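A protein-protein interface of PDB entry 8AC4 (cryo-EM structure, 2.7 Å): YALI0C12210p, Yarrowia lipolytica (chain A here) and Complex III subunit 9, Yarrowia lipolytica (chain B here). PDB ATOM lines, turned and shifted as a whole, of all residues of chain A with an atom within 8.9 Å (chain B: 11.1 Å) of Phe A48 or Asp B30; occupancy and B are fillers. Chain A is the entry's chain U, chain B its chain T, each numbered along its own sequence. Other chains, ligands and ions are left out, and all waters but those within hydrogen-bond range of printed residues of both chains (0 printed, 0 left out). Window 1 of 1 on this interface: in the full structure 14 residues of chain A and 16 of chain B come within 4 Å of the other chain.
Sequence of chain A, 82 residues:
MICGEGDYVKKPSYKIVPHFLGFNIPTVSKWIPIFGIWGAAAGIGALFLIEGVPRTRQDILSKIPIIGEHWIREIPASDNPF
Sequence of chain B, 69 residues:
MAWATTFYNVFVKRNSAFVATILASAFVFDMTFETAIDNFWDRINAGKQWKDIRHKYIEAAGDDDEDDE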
ATOM      1  N   ALA A  40      23.323  -6.663  23.578  1.00  0.00           N
ATOM      2  CA  ALA A  40      23.541  -6.674  22.143  1.00  0.00           C
ATOM      3  C   ALA A  40      22.559  -7.628  21.467  1.00  0.00           C
ATOM      4  O   ALA A  40      21.951  -7.261  20.472  1.00  0.00           O
ATOM      5  CB  ALA A  40      24.967  -7.036  21.822  1.00  0.00           C
ATOM      6  N   ALA A  41      22.420  -8.846  22.006  1.00  0.00           N
ATOM      7  CA  ALA A  41      21.494  -9.824  21.459  1.00  0.00           C
ATOM      8  C   ALA A  41      20.085  -9.237  21.445  1.00  0.00           C
ATOM      9  O   ALA A  41      19.354  -9.436  20.480  1.00  0.00           O
ATOM     10  CB  ALA A  41      21.549 -11.117  22.237  1.00  0.00           C
ATOM     11  N   ALA A  42      19.726  -8.533  22.527  1.00  0.00           N
ATOM     12  CA  ALA A  42      18.396  -7.964  22.658  1.00  0.00           C
ATOM     13  C   ALA A  42      18.235  -6.797  21.688  1.00  0.00           C
ATOM     14  O   ALA A  42      17.174  -6.640  21.089  1.00  0.00           O
ATOM     15  CB  ALA A  42      18.113  -7.565  24.085  1.00  0.00           C
ATOM     16  N   GLY A  43      19.313  -6.019  21.516  1.00  0.00           N
ATOM     17  CA  GLY A  43      19.333  -4.894  20.597  1.00  0.00           C
ATOM     18  C   GLY A  43      19.169  -5.351  19.150  1.00  0.00           C
ATOM     19  O   GLY A  43      18.273  -4.872  18.458  1.00  0.00           O
ATOM     20  N   ILE A  44      20.045  -6.275  18.719  1.00  0.00           N
ATOM     21  CA  ILE A  44      20.004  -6.856  17.383  1.00  0.00           C
ATOM     22  C   ILE A  44      18.611  -7.438  17.154  1.00  0.00           C
ATOM     23  O   ILE A  44      18.004  -7.173  16.122  1.00  0.00           O
ATOM     24  CB  ILE A  44      21.114  -7.914  17.174  1.00  0.00           C
ATOM     25  CG1 ILE A  44      22.519  -7.305  17.229  1.00  0.00           C
ATOM     26  CG2 ILE A  44      20.901  -8.693  15.880  1.00  0.00           C
ATOM     27  CD1 ILE A  44      23.614  -8.294  17.600  1.00  0.00           C
ATOM     28  N   GLY A  45      18.120  -8.210  18.134  1.00  0.00           N
ATOM     29  CA  GLY A  45      16.842  -8.892  18.012  1.00  0.00           C
ATOM     30  C   GLY A  45      15.669  -7.919  17.892  1.00  0.00           C
ATOM     31  O   GLY A  45      14.775  -8.119  17.067  1.00  0.00           O
ATOM     32  N   ALA A  46      15.686  -6.871  18.726  1.00  0.00           N
ATOM     33  CA  ALA A  46      14.590  -5.916  18.743  1.00  0.00           C
ATOM     34  C   ALA A  46      14.552  -5.185  17.407  1.00  0.00           C
ATOM     35  O   ALA A  46      13.494  -5.079  16.786  1.00  0.00           O
ATOM     36  CB  ALA A  46      14.729  -4.961  19.904  1.00  0.00           C
ATOM     37  N   LEU A  47      15.734  -4.755  16.957  1.00  0.00           N
ATOM     38  CA  LEU A  47      15.851  -3.969  15.744  1.00  0.00           C
ATOM     39  C   LEU A  47      15.422  -4.814  14.547  1.00  0.00           C
ATOM     40  O   LEU A  47      14.777  -4.307  13.632  1.00  0.00           O
ATOM     41  CB  LEU A  47      17.298  -3.487  15.607  1.00  0.00           C
ATOM     42  CG  LEU A  47      17.639  -2.767  14.304  1.00  0.00           C
ATOM     43  CD1 LEU A  47      17.047  -1.364  14.277  1.00  0.00           C
ATOM     44  CD2 LEU A  47      19.147  -2.710  14.110  1.00  0.00           C
ATOM     45  N   PHE A  48      15.778  -6.100  14.590  1.00  0.00           N
ATOM     46  CA  PHE A  48      15.398  -7.077  13.588  1.00  0.00           C
ATOM     47  C   PHE A  48      13.881  -7.216  13.517  1.00  0.00           C
ATOM     48  O   PHE A  48      13.333  -7.327  12.424  1.00  0.00           O
ATOM     49  CB  PHE A  48      16.045  -8.417  13.933  1.00  0.00           C
ATOM     50  CG  PHE A  48      15.801  -9.525  12.944  1.00  0.00           C
ATOM     51  CD1 PHE A  48      15.869  -9.294  11.573  1.00  0.00           C
ATOM     52  CD2 PHE A  48      15.527 -10.812  13.388  1.00  0.00           C
ATOM     53  CE1 PHE A  48      15.648 -10.324  10.667  1.00  0.00           C
ATOM     54  CE2 PHE A  48      15.318 -11.843  12.482  1.00  0.00           C
ATOM     55  CZ  PHE A  48      15.378 -11.599  11.124  1.00  0.00           C
ATOM     56  N   LEU A  49      13.216  -7.216  14.681  1.00  0.00           N
ATOM     57  CA  LEU A  49      11.770  -7.382  14.734  1.00  0.00           C
ATOM     58  C   LEU A  49      11.046  -6.178  14.144  1.00  0.00           C
ATOM     59  O   LEU A  49       9.926  -6.308  13.655  1.00  0.00           O
ATOM     60  CB  LEU A  49      11.312  -7.585  16.177  1.00  0.00           C
ATOM     61  CG  LEU A  49      11.325  -9.028  16.671  1.00  0.00           C
ATOM     62  CD1 LEU A  49      10.940  -9.069  18.138  1.00  0.00           C
ATOM     63  CD2 LEU A  49      10.392  -9.911  15.852  1.00  0.00           C
ATOM     64  N   ILE A  50      11.661  -4.997  14.229  1.00  0.00           N
ATOM     65  CA  ILE A  50      10.959  -3.819  13.749  1.00  0.00           C
ATOM     66  C   ILE A  50      11.595  -3.297  12.469  1.00  0.00           C
ATOM     67  O   ILE A  50      11.393  -2.143  12.100  1.00  0.00           O
ATOM     68  CB  ILE A  50      10.871  -2.729  14.826  1.00  0.00           C
ATOM     69  CG1 ILE A  50      12.264  -2.266  15.268  1.00  0.00           C
ATOM     70  CG2 ILE A  50       9.972  -3.184  15.970  1.00  0.00           C
ATOM     71  CD1 ILE A  50      12.282  -0.933  15.976  1.00  0.00           C
ATOM     72  N   GLU A  51      12.341  -4.159  11.786  1.00  0.00           N
ATOM     73  CA  GLU A  51      13.043  -3.749  10.585  1.00  0.00           C
ATOM     74  C   GLU A  51      12.016  -3.319   9.539  1.00  0.00           C
ATOM     75  O   GLU A  51      12.295  -2.474   8.694  1.00  0.00           O
ATOM     76  CB  GLU A  51      13.927  -4.907  10.124  1.00  0.00           C
ATOM     77  CG  GLU A  51      14.561  -4.728   8.748  1.00  0.00           C
ATOM     78  CD  GLU A  51      13.724  -5.020   7.506  1.00  0.00           C
ATOM     79  OE1 GLU A  51      12.845  -5.917   7.553  1.00  0.00           O
ATOM     80  OE2 GLU A  51      13.966  -4.358   6.470  1.00  0.00           O
ATOM     81  N   GLY A  52      10.837  -3.939   9.599  1.00  0.00           N
ATOM     82  CA  GLY A  52       9.785  -3.685   8.634  1.00  0.00           C
ATOM     83  C   GLY A  52       9.086  -2.345   8.867  1.00  0.00           C
ATOM     84  O   GLY A  52       8.625  -1.724   7.911  1.00  0.00           O
ATOM     85  N   VAL A  53       9.015  -1.907  10.127  1.00  0.00           N
ATOM     86  CA  VAL A  53       8.415  -0.627  10.465  1.00  0.00           C
ATOM     87  C   VAL A  53       9.083   0.488   9.660  1.00  0.00           C
ATOM     88  O   VAL A  53      10.298   0.641   9.709  1.00  0.00           O
ATOM     89  CB  VAL A  53       8.509  -0.364  11.973  1.00  0.00           C
ATOM     90  CG1 VAL A  53       7.964   1.008  12.344  1.00  0.00           C
ATOM     91  CG2 VAL A  53       7.816  -1.468  12.751  1.00  0.00           C
ATOM     92  N   THR A  56      11.579   2.796  11.424  1.00  0.00           N
ATOM     93  CA  THR A  56      12.861   2.169  11.716  1.00  0.00           C
ATOM     94  C   THR A  56      13.801   2.330  10.529  1.00  0.00           C
ATOM     95  O   THR A  56      14.997   2.501  10.719  1.00  0.00           O
ATOM     96  CB  THR A  56      12.707   0.660  11.931  1.00  0.00           C
ATOM     97  OG1 THR A  56      11.691   0.519  12.919  1.00  0.00           O
ATOM     98  CG2 THR A  56      13.975  -0.048  12.364  1.00  0.00           C
ATOM     99  N   ARG A  57      13.258   2.232   9.314  1.00  0.00           N
ATOM    100  CA  ARG A  57      14.087   2.298   8.128  1.00  0.00           C
ATOM    101  C   ARG A  57      14.535   3.733   7.934  1.00  0.00           C
ATOM    102  O   ARG A  57      15.721   3.985   7.758  1.00  0.00           O
ATOM    103  CB  ARG A  57      13.306   1.804   6.916  1.00  0.00           C
ATOM    104  CG  ARG A  57      13.051   0.311   6.980  1.00  0.00           C
ATOM    105  CD  ARG A  57      12.021  -0.076   5.954  1.00  0.00           C
ATOM    106  NE  ARG A  57      11.842  -1.510   6.051  1.00  0.00           N
ATOM    107  CZ  ARG A  57      11.262  -2.221   5.105  1.00  0.00           C
ATOM    108  NH1 ARG A  57      10.816  -1.616   4.018  1.00  0.00           N
ATOM    109  NH2 ARG A  57      11.128  -3.526   5.239  1.00  0.00           N
ATOM    110  N   LEU A  61      17.894   2.498   9.957  1.00  0.00           N
ATOM    111  CA  LEU A  61      18.546   1.572   9.048  1.00  0.00           C
ATOM    112  C   LEU A  61      19.118   2.260   7.810  1.00  0.00           C
ATOM    113  O   LEU A  61      20.143   1.817   7.307  1.00  0.00           O
ATOM    114  CB  LEU A  61      17.576   0.449   8.682  1.00  0.00           C
ATOM    115  CG  LEU A  61      17.235  -0.490   9.837  1.00  0.00           C
ATOM    116  CD1 LEU A  61      16.177  -1.498   9.432  1.00  0.00           C
ATOM    117  CD2 LEU A  61      18.478  -1.192  10.370  1.00  0.00           C
ATOM    118  N   HIS A  70      20.061  -0.094   1.161  1.00  0.00           N
ATOM    119  CA  HIS A  70      19.185  -1.250   1.058  1.00  0.00           C
ATOM    120  C   HIS A  70      17.758  -0.861   1.445  1.00  0.00           C
ATOM    121  O   HIS A  70      16.808  -1.472   0.965  1.00  0.00           O
ATOM    122  CB  HIS A  70      19.745  -2.426   1.873  1.00  0.00           C
ATOM    123  CG  HIS A  70      18.813  -3.585   1.980  1.00  0.00           C
ATOM    124  ND1 HIS A  70      18.658  -4.513   0.967  1.00  0.00           N
ATOM    125  CD2 HIS A  70      17.974  -3.964   2.970  1.00  0.00           C
ATOM    126  CE1 HIS A  70      17.763  -5.410   1.331  1.00  0.00           C
ATOM    127  NE2 HIS A  70      17.330  -5.097   2.557  1.00  0.00           N
ATOM    128  N   TRP A  71      17.627   0.164   2.297  1.00  0.00           N
ATOM    129  CA  TRP A  71      16.343   0.503   2.889  1.00  0.00           C
ATOM    130  C   TRP A  71      15.769   1.802   2.332  1.00  0.00           C
ATOM    131  O   TRP A  71      14.727   2.264   2.799  1.00  0.00           O
ATOM    132  CB  TRP A  71      16.463   0.582   4.403  1.00  0.00           C
ATOM    133  CG  TRP A  71      16.654  -0.751   5.044  1.00  0.00           C
ATOM    134  CD1 TRP A  71      15.700  -1.690   5.305  1.00  0.00           C
ATOM    135  CD2 TRP A  71      17.891  -1.289   5.526  1.00  0.00           C
ATOM    136  NE1 TRP A  71      16.260  -2.776   5.917  1.00  0.00           N
ATOM    137  CE2 TRP A  71      17.600  -2.559   6.072  1.00  0.00           C
ATOM    138  CE3 TRP A  71      19.209  -0.818   5.551  1.00  0.00           C
ATOM    139  CZ2 TRP A  71      18.579  -3.363   6.649  1.00  0.00           C
ATOM    140  CZ3 TRP A  71      20.175  -1.609   6.129  1.00  0.00           C
ATOM    141  CH2 TRP A  71      19.864  -2.867   6.654  1.00  0.00           C
ATOM    142  N   ARG A  73      14.014   2.795  -0.619  1.00  0.00           N
ATOM    143  CA  ARG A  73      13.324   2.251  -1.779  1.00  0.00           C
ATOM    144  C   ARG A  73      12.058   3.057  -2.054  1.00  0.00           C
ATOM    145  O   ARG A  73      11.244   3.269  -1.156  1.00  0.00           O
ATOM    146  CB  ARG A  73      13.054   0.752  -1.608  1.00  0.00           C
ATOM    147  CG  ARG A  73      12.718   0.334  -0.186  1.00  0.00           C
ATOM    148  CD  ARG A  73      12.128  -1.057  -0.111  1.00  0.00           C
ATOM    149  NE  ARG A  73      12.520  -1.708   1.133  1.00  0.00           N
ATOM    150  CZ  ARG A  73      13.441  -2.663   1.241  1.00  0.00           C
ATOM    151  NH1 ARG A  73      14.072  -3.112   0.169  1.00  0.00           N
ATOM    152  NH2 ARG A  73      13.717  -3.180   2.426  1.00  0.00           N
ATOM    153  N   VAL B  19      23.592 -16.775  20.867  1.00  0.00           N
ATOM    154  CA  VAL B  19      22.286 -16.263  20.505  1.00  0.00           C
ATOM    155  C   VAL B  19      22.470 -14.962  19.732  1.00  0.00           C
ATOM    156  O   VAL B  19      21.783 -14.743  18.747  1.00  0.00           O
ATOM    157  CB  VAL B  19      21.357 -16.100  21.721  1.00  0.00           C
ATOM    158  CG1 VAL B  19      20.138 -15.275  21.354  1.00  0.00           C
ATOM    159  CG2 VAL B  19      20.893 -17.451  22.240  1.00  0.00           C
ATOM    160  N   ALA B  20      23.419 -14.125  20.160  1.00  0.00           N
ATOM    161  CA  ALA B  20      23.686 -12.887  19.442  1.00  0.00           C
ATOM    162  C   ALA B  20      24.138 -13.171  18.009  1.00  0.00           C
ATOM    163  O   ALA B  20      23.729 -12.463  17.097  1.00  0.00           O
ATOM    164  CB  ALA B  20      24.668 -12.011  20.185  1.00  0.00           C
ATOM    165  N   THR B  21      24.972 -14.198  17.819  1.00  0.00           N
ATOM    166  CA  THR B  21      25.476 -14.556  16.502  1.00  0.00           C
ATOM    167  C   THR B  21      24.346 -15.087  15.624  1.00  0.00           C
ATOM    168  O   THR B  21      24.297 -14.774  14.441  1.00  0.00           O
ATOM    169  CB  THR B  21      26.613 -15.575  16.616  1.00  0.00           C
ATOM    170  OG1 THR B  21      27.615 -14.966  17.426  1.00  0.00           O
ATOM    171  CG2 THR B  21      27.212 -15.953  15.279  1.00  0.00           C
ATOM    172  N   ILE B  22      23.460 -15.901  16.208  1.00  0.00           N
ATOM    173  CA  ILE B  22      22.320 -16.460  15.495  1.00  0.00           C
ATOM    174  C   ILE B  22      21.419 -15.317  15.025  1.00  0.00           C
ATOM    175  O   ILE B  22      21.030 -15.311  13.866  1.00  0.00           O
ATOM    176  CB  ILE B  22      21.574 -17.512  16.350  1.00  0.00           C
ATOM    177  CG1 ILE B  22      22.347 -18.833  16.437  1.00  0.00           C
ATOM    178  CG2 ILE B  22      20.140 -17.735  15.875  1.00  0.00           C
ATOM    179  CD1 ILE B  22      22.012 -19.677  17.661  1.00  0.00           C
ATOM    180  N   LEU B  23      21.099 -14.363  15.913  1.00  0.00           N
ATOM    181  CA  LEU B  23      20.199 -13.274  15.559  1.00  0.00           C
ATOM    182  C   LEU B  23      20.818 -12.363  14.508  1.00  0.00           C
ATOM    183  O   LEU B  23      20.113 -11.922  13.606  1.00  0.00           O
ATOM    184  CB  LEU B  23      19.770 -12.484  16.796  1.00  0.00           C
ATOM    185  CG  LEU B  23      18.937 -13.289  17.790  1.00  0.00           C
ATOM    186  CD1 LEU B  23      18.600 -12.471  19.025  1.00  0.00           C
ATOM    187  CD2 LEU B  23      17.684 -13.847  17.135  1.00  0.00           C
ATOM    188  N   ALA B  24      22.120 -12.084  14.620  1.00  0.00           N
ATOM    189  CA  ALA B  24      22.754 -11.235  13.627  1.00  0.00           C
ATOM    190  C   ALA B  24      22.781 -11.947  12.275  1.00  0.00           C
ATOM    191  O   ALA B  24      22.592 -11.325  11.238  1.00  0.00           O
ATOM    192  CB  ALA B  24      24.130 -10.835  14.082  1.00  0.00           C
ATOM    193  N   SER B  25      22.998 -13.261  12.298  1.00  0.00           N
ATOM    194  CA  SER B  25      22.986 -14.051  11.080  1.00  0.00           C
ATOM    195  C   SER B  25      21.589 -14.058  10.466  1.00  0.00           C
ATOM    196  O   SER B  25      21.455 -14.018   9.252  1.00  0.00           O
ATOM    197  CB  SER B  25      23.434 -15.438  11.373  1.00  0.00           C
ATOM    198  OG  SER B  25      24.764 -15.431  11.860  1.00  0.00           O
ATOM    199  N   ALA B  26      20.566 -14.139  11.323  1.00  0.00           N
ATOM    200  CA  ALA B  26      19.183 -14.135  10.878  1.00  0.00           C
ATOM    201  C   ALA B  26      18.872 -12.820  10.168  1.00  0.00           C
ATOM    202  O   ALA B  26      18.211 -12.838   9.137  1.00  0.00           O
ATOM    203  CB  ALA B  26      18.258 -14.385  12.043  1.00  0.00           C
ATOM    204  N   PHE B  27      19.351 -11.705  10.731  1.00  0.00           N
ATOM    205  CA  PHE B  27      19.192 -10.391  10.134  1.00  0.00           C
ATOM    206  C   PHE B  27      19.822 -10.379   8.745  1.00  0.00           C
ATOM    207  O   PHE B  27      19.177  -9.962   7.786  1.00  0.00           O
ATOM    208  CB  PHE B  27      19.839  -9.322  11.015  1.00  0.00           C
ATOM    209  CG  PHE B  27      19.200  -7.956  10.980  1.00  0.00           C
ATOM    210  CD1 PHE B  27      18.796  -7.363   9.788  1.00  0.00           C
ATOM    211  CD2 PHE B  27      19.025  -7.240  12.155  1.00  0.00           C
ATOM    212  CE1 PHE B  27      18.208  -6.106   9.775  1.00  0.00           C
ATOM    213  CE2 PHE B  27      18.449  -5.975  12.146  1.00  0.00           C
ATOM    214  CZ  PHE B  27      18.039  -5.411  10.955  1.00  0.00           C
ATOM    215  N   VAL B  28      21.060 -10.868   8.636  1.00  0.00           N
ATOM    216  CA  VAL B  28      21.759 -10.815   7.363  1.00  0.00           C
ATOM    217  C   VAL B  28      21.083 -11.744   6.360  1.00  0.00           C
ATOM    218  O   VAL B  28      20.879 -11.369   5.209  1.00  0.00           O
ATOM    219  CB  VAL B  28      23.245 -11.160   7.525  1.00  0.00           C
ATOM    220  CG1 VAL B  28      23.917 -11.372   6.181  1.00  0.00           C
ATOM    221  CG2 VAL B  28      23.966 -10.095   8.330  1.00  0.00           C
ATOM    222  N   PHE B  29      20.751 -12.957   6.801  1.00  0.00           N
ATOM    223  CA  PHE B  29      20.085 -13.904   5.926  1.00  0.00           C
ATOM    224  C   PHE B  29      18.800 -13.279   5.396  1.00  0.00           C
ATOM    225  O   PHE B  29      18.573 -13.249   4.194  1.00  0.00           O
ATOM    226  CB  PHE B  29      19.765 -15.199   6.673  1.00  0.00           C
ATOM    227  CG  PHE B  29      18.892 -16.129   5.874  1.00  0.00           C
ATOM    228  CD1 PHE B  29      19.445 -16.942   4.896  1.00  0.00           C
ATOM    229  CD2 PHE B  29      17.515 -16.157   6.060  1.00  0.00           C
ATOM    230  CE1 PHE B  29      18.644 -17.789   4.143  1.00  0.00           C
ATOM    231  CE2 PHE B  29      16.713 -16.998   5.299  1.00  0.00           C
ATOM    232  CZ  PHE B  29      17.279 -17.810   4.339  1.00  0.00           C
ATOM    233  N   ASP B  30      17.971 -12.772   6.308  1.00  0.00           N
ATOM    234  CA  ASP B  30      16.699 -12.174   5.944  1.00  0.00           C
ATOM    235  C   ASP B  30      16.866 -11.144   4.825  1.00  0.00           C
ATOM    236  O   ASP B  30      16.064 -11.127   3.900  1.00  0.00           O
ATOM    237  CB  ASP B  30      16.022 -11.560   7.169  1.00  0.00           C
ATOM    238  CG  ASP B  30      14.513 -11.445   7.035  1.00  0.00           C
ATOM    239  OD1 ASP B  30      13.832 -12.491   7.142  1.00  0.00           O
ATOM    240  OD2 ASP B  30      14.020 -10.316   6.835  1.00  0.00           O
ATOM    241  N   MET B  31      17.876 -10.272   4.935  1.00  0.00           N
ATOM    242  CA  MET B  31      18.054  -9.159   4.013  1.00  0.00           C
ATOM    243  C   MET B  31      18.552  -9.636   2.654  1.00  0.00           C
ATOM    244  O   MET B  31      18.096  -9.164   1.611  1.00  0.00           O
ATOM    245  CB  MET B  31      19.037  -8.136   4.591  1.00  0.00           C
ATOM    246  CG  MET B  31      18.495  -7.383   5.793  1.00  0.00           C
ATOM    247  SD  MET B  31      16.865  -6.663   5.491  1.00  0.00           S
ATOM    248  CE  MET B  31      15.816  -7.806   6.388  1.00  0.00           C
ATOM    249  N   THR B  32      19.490 -10.577   2.685  1.00  0.00           N
ATOM    250  CA  THR B  32      20.129 -11.040   1.471  1.00  0.00           C
ATOM    251  C   THR B  32      19.201 -11.991   0.733  1.00  0.00           C
ATOM    252  O   THR B  32      19.162 -11.961  -0.488  1.00  0.00           O
ATOM    253  CB  THR B  32      21.484 -11.669   1.782  1.00  0.00           C
ATOM    254  OG1 THR B  32      21.229 -12.668   2.768  1.00  0.00           O
ATOM    255  CG2 THR B  32      22.462 -10.650   2.320  1.00  0.00           C
ATOM    256  N   PHE B  33      18.446 -12.805   1.476  1.00  0.00           N
ATOM    257  CA  PHE B  33      17.581 -13.804   0.872  1.00  0.00           C
ATOM    258  C   PHE B  33      16.445 -13.109   0.135  1.00  0.00           C
ATOM    259  O   PHE B  33      16.042 -13.551  -0.935  1.00  0.00           O
ATOM    260  CB  PHE B  33      17.041 -14.741   1.953  1.00  0.00           C
ATOM    261  CG  PHE B  33      16.124 -15.845   1.496  1.00  0.00           C
ATOM    262  CD1 PHE B  33      16.566 -16.828   0.616  1.00  0.00           C
ATOM    263  CD2 PHE B  33      14.838 -15.953   2.013  1.00  0.00           C
ATOM    264  CE1 PHE B  33      15.733 -17.873   0.237  1.00  0.00           C
ATOM    265  CE2 PHE B  33      14.001 -16.993   1.627  1.00  0.00           C
ATOM    266  CZ  PHE B  33      14.451 -17.955   0.744  1.00  0.00           C
ATOM    267  N   GLU B  34      15.954 -12.023   0.736  1.00  0.00           N
ATOM    268  CA  GLU B  34      14.929 -11.180   0.149  1.00  0.00           C
ATOM    269  C   GLU B  34      15.409 -10.712  -1.220  1.00  0.00           C
ATOM    270  O   GLU B  34      14.709 -10.888  -2.208  1.00  0.00           O
ATOM    271  CB  GLU B  34      14.648 -10.013   1.099  1.00  0.00           C
ATOM    272  CG  GLU B  34      13.504  -9.099   0.682  1.00  0.00           C
ATOM    273  CD  GLU B  34      13.877  -7.725   0.138  1.00  0.00           C
ATOM    274  OE1 GLU B  34      12.966  -6.875   0.017  1.00  0.00           O
ATOM    275  OE2 GLU B  34      15.070  -7.506  -0.175  1.00  0.00           O
ATOM    276  N   THR B  35      16.604 -10.123  -1.253  1.00  0.00           N
ATOM    277  CA  THR B  35      17.176  -9.569  -2.464  1.00  0.00           C
ATOM    278  C   THR B  35      17.404 -10.654  -3.508  1.00  0.00           C
ATOM    279  O   THR B  35      17.188 -10.415  -4.688  1.00  0.00           O
ATOM    280  CB  THR B  35      18.487  -8.864  -2.131  1.00  0.00           C
ATOM    281  OG1 THR B  35      18.017  -7.714  -1.434  1.00  0.00           O
ATOM    282  CG2 THR B  35      19.293  -8.491  -3.355  1.00  0.00           C
ATOM    283  N   ALA B  36      17.849 -11.831  -3.071  1.00  0.00           N
ATOM    284  CA  ALA B  36      18.213 -12.900  -3.987  1.00  0.00           C
ATOM    285  C   ALA B  36      16.968 -13.478  -4.648  1.00  0.00           C
ATOM    286  O   ALA B  36      16.994 -13.792  -5.836  1.00  0.00           O
ATOM    287  CB  ALA B  36      18.984 -13.964  -3.251  1.00  0.00           C
ATOM    288  N   ILE B  37      15.900 -13.632  -3.855  1.00  0.00           N
ATOM    289  CA  ILE B  37      14.672 -14.208  -4.370  1.00  0.00           C
ATOM    290  C   ILE B  37      14.049 -13.209  -5.334  1.00  0.00           C
ATOM    291  O   ILE B  37      13.689 -13.595  -6.440  1.00  0.00           O
ATOM    292  CB  ILE B  37      13.720 -14.668  -3.245  1.00  0.00           C
ATOM    293  CG1 ILE B  37      14.253 -15.919  -2.541  1.00  0.00           C
ATOM    294  CG2 ILE B  37      12.294 -14.878  -3.752  1.00  0.00           C
ATOM    295  CD1 ILE B  37      14.567 -17.083  -3.468  1.00  0.00           C
ATOM    296  N   ASP B  38      14.001 -11.934  -4.928  1.00  0.00           N
ATOM    297  CA  ASP B  38      13.524 -10.865  -5.791  1.00  0.00           C
ATOM    298  C   ASP B  38      14.160 -10.971  -7.177  1.00  0.00           C
ATOM    299  O   ASP B  38      13.436 -10.968  -8.165  1.00  0.00           O
ATOM    300  CB  ASP B  38      13.731  -9.463  -5.204  1.00  0.00           C
ATOM    301  CG  ASP B  38      12.840  -9.086  -4.024  1.00  0.00           C
ATOM    302  OD1 ASP B  38      11.966  -9.894  -3.646  1.00  0.00           O
ATOM    303  OD2 ASP B  38      13.042  -7.978  -3.470  1.00  0.00           O
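A ring nitrogen (NE2) of His A70 sits at hydrogen-bond distance from the side-chain sulfur of Met B31, 3.4 Å away. The guanidinium group (NH1) of Arg A73 lies within salt-bridge range of the side-chain carboxylate (OE1) of Glu B34 (3.9 Å).
OE2 of Glu A51 lies within salt-bridge range of NH2 of Arg A57, 3.2 Å away. The side-chain hydroxyl of Thr B35 lies within hydrogen-bond range of the backbone carbonyl oxygen of Met B31. OE2 of Glu A51 sits at hydrogen-bond distance from NE1 of Trp A71, 2.8 Å away. The backbone carbonyl oxygen (O) of His A70 lies within hydrogen-bond range of the guanidinium group (NH1) of Arg A73. The side-chain hydroxyl (OG1) of Thr B35 lies within hydrogen-bond range of the side-chain carboxylate (OE2) of Glu B34.
Ala B20 touches Ala A41 (CB to CB, 3.8 Å). Leu B23 touches Ala A41. Ile A44 touches Leu B23. Leu A47 touches Phe B27. O of Ala B26 touches CZ of Phe A48, at 3.7 Å. Phe B27 touches Phe A48. Phe A48 touches Asp B30 (CE1 to CB, 3.7 Å). Glu A51 touches Met B31. Thr B35 touches His A70. Trp A71 touches Met B31 (CZ2 to SD, 3.9 Å).
Printed residues of chain B within 4 Å of Ala A41: Ala B20 and Leu B23. Printed residues of chain B within 4 Å of Ile A44: Leu B23 and Ala B24. Gly A45 touches none of the printed residues of chain B. Of chain B, only Phe B27 (3.9 Å) comes within 4 Å of Leu A47. Of chain B, only Ala B26, Phe B27 and Asp B30 come within 4 Å of Phe A48. No residue of chain B comes within 4 Å of Leu A49. No residue of chain B comes within 4 Å of Ile A50. Of chain B, only Met B31 comes within 4 Å of Glu A51. Printed residues of chain A within 4 Å of Ala B20: Ala A41 (3.8 Å). Printed residues of chain A within 4 Å of Leu B23: Ala A41 and Ile A44. Of the printed residues of chain A, Ala B24 touches Ile A44 (3.8 Å). Of chain A, only Leu A47 and Phe A48 come within 4 Å of Phe B27. Met B31 touches just these residues of chain A: Glu A51, His A70 and Trp A71. The nearest residue of chain B that does not touch Phe A48 is Leu B23 (4.7 Å). The nearest residue of chain A that does not touch Asp B30 is Glu A51 (4.6 Å). The nearest printed residue of chain A that does not touch Leu B23 is Gly A45 (4.1 Å).
Of the 20 printed residues of chain A, 8 touch a printed residue of chain B. Hydrophobic or aromatic side chains of chain A that line the printed part of chain B: Ala A41, Ile A44, Leu A47, Phe A48, His A70 and Trp A71. Printed residues of chain B that touch a printed residue of chain A: Ala B20, Leu B23, Ala B24, Ala B26, Phe B27, Asp B30, Met B31, Glu B34 and Thr B35. Along chain B the printed residues that touch a printed residue of chain A span positions 20 to 35. Among the printed residues, Asp or Glu carboxylates within 4 Å of a Lys or Arg side-chain nitrogen of the other chain: Arg A73 with Glu B34 (3.9 Å).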
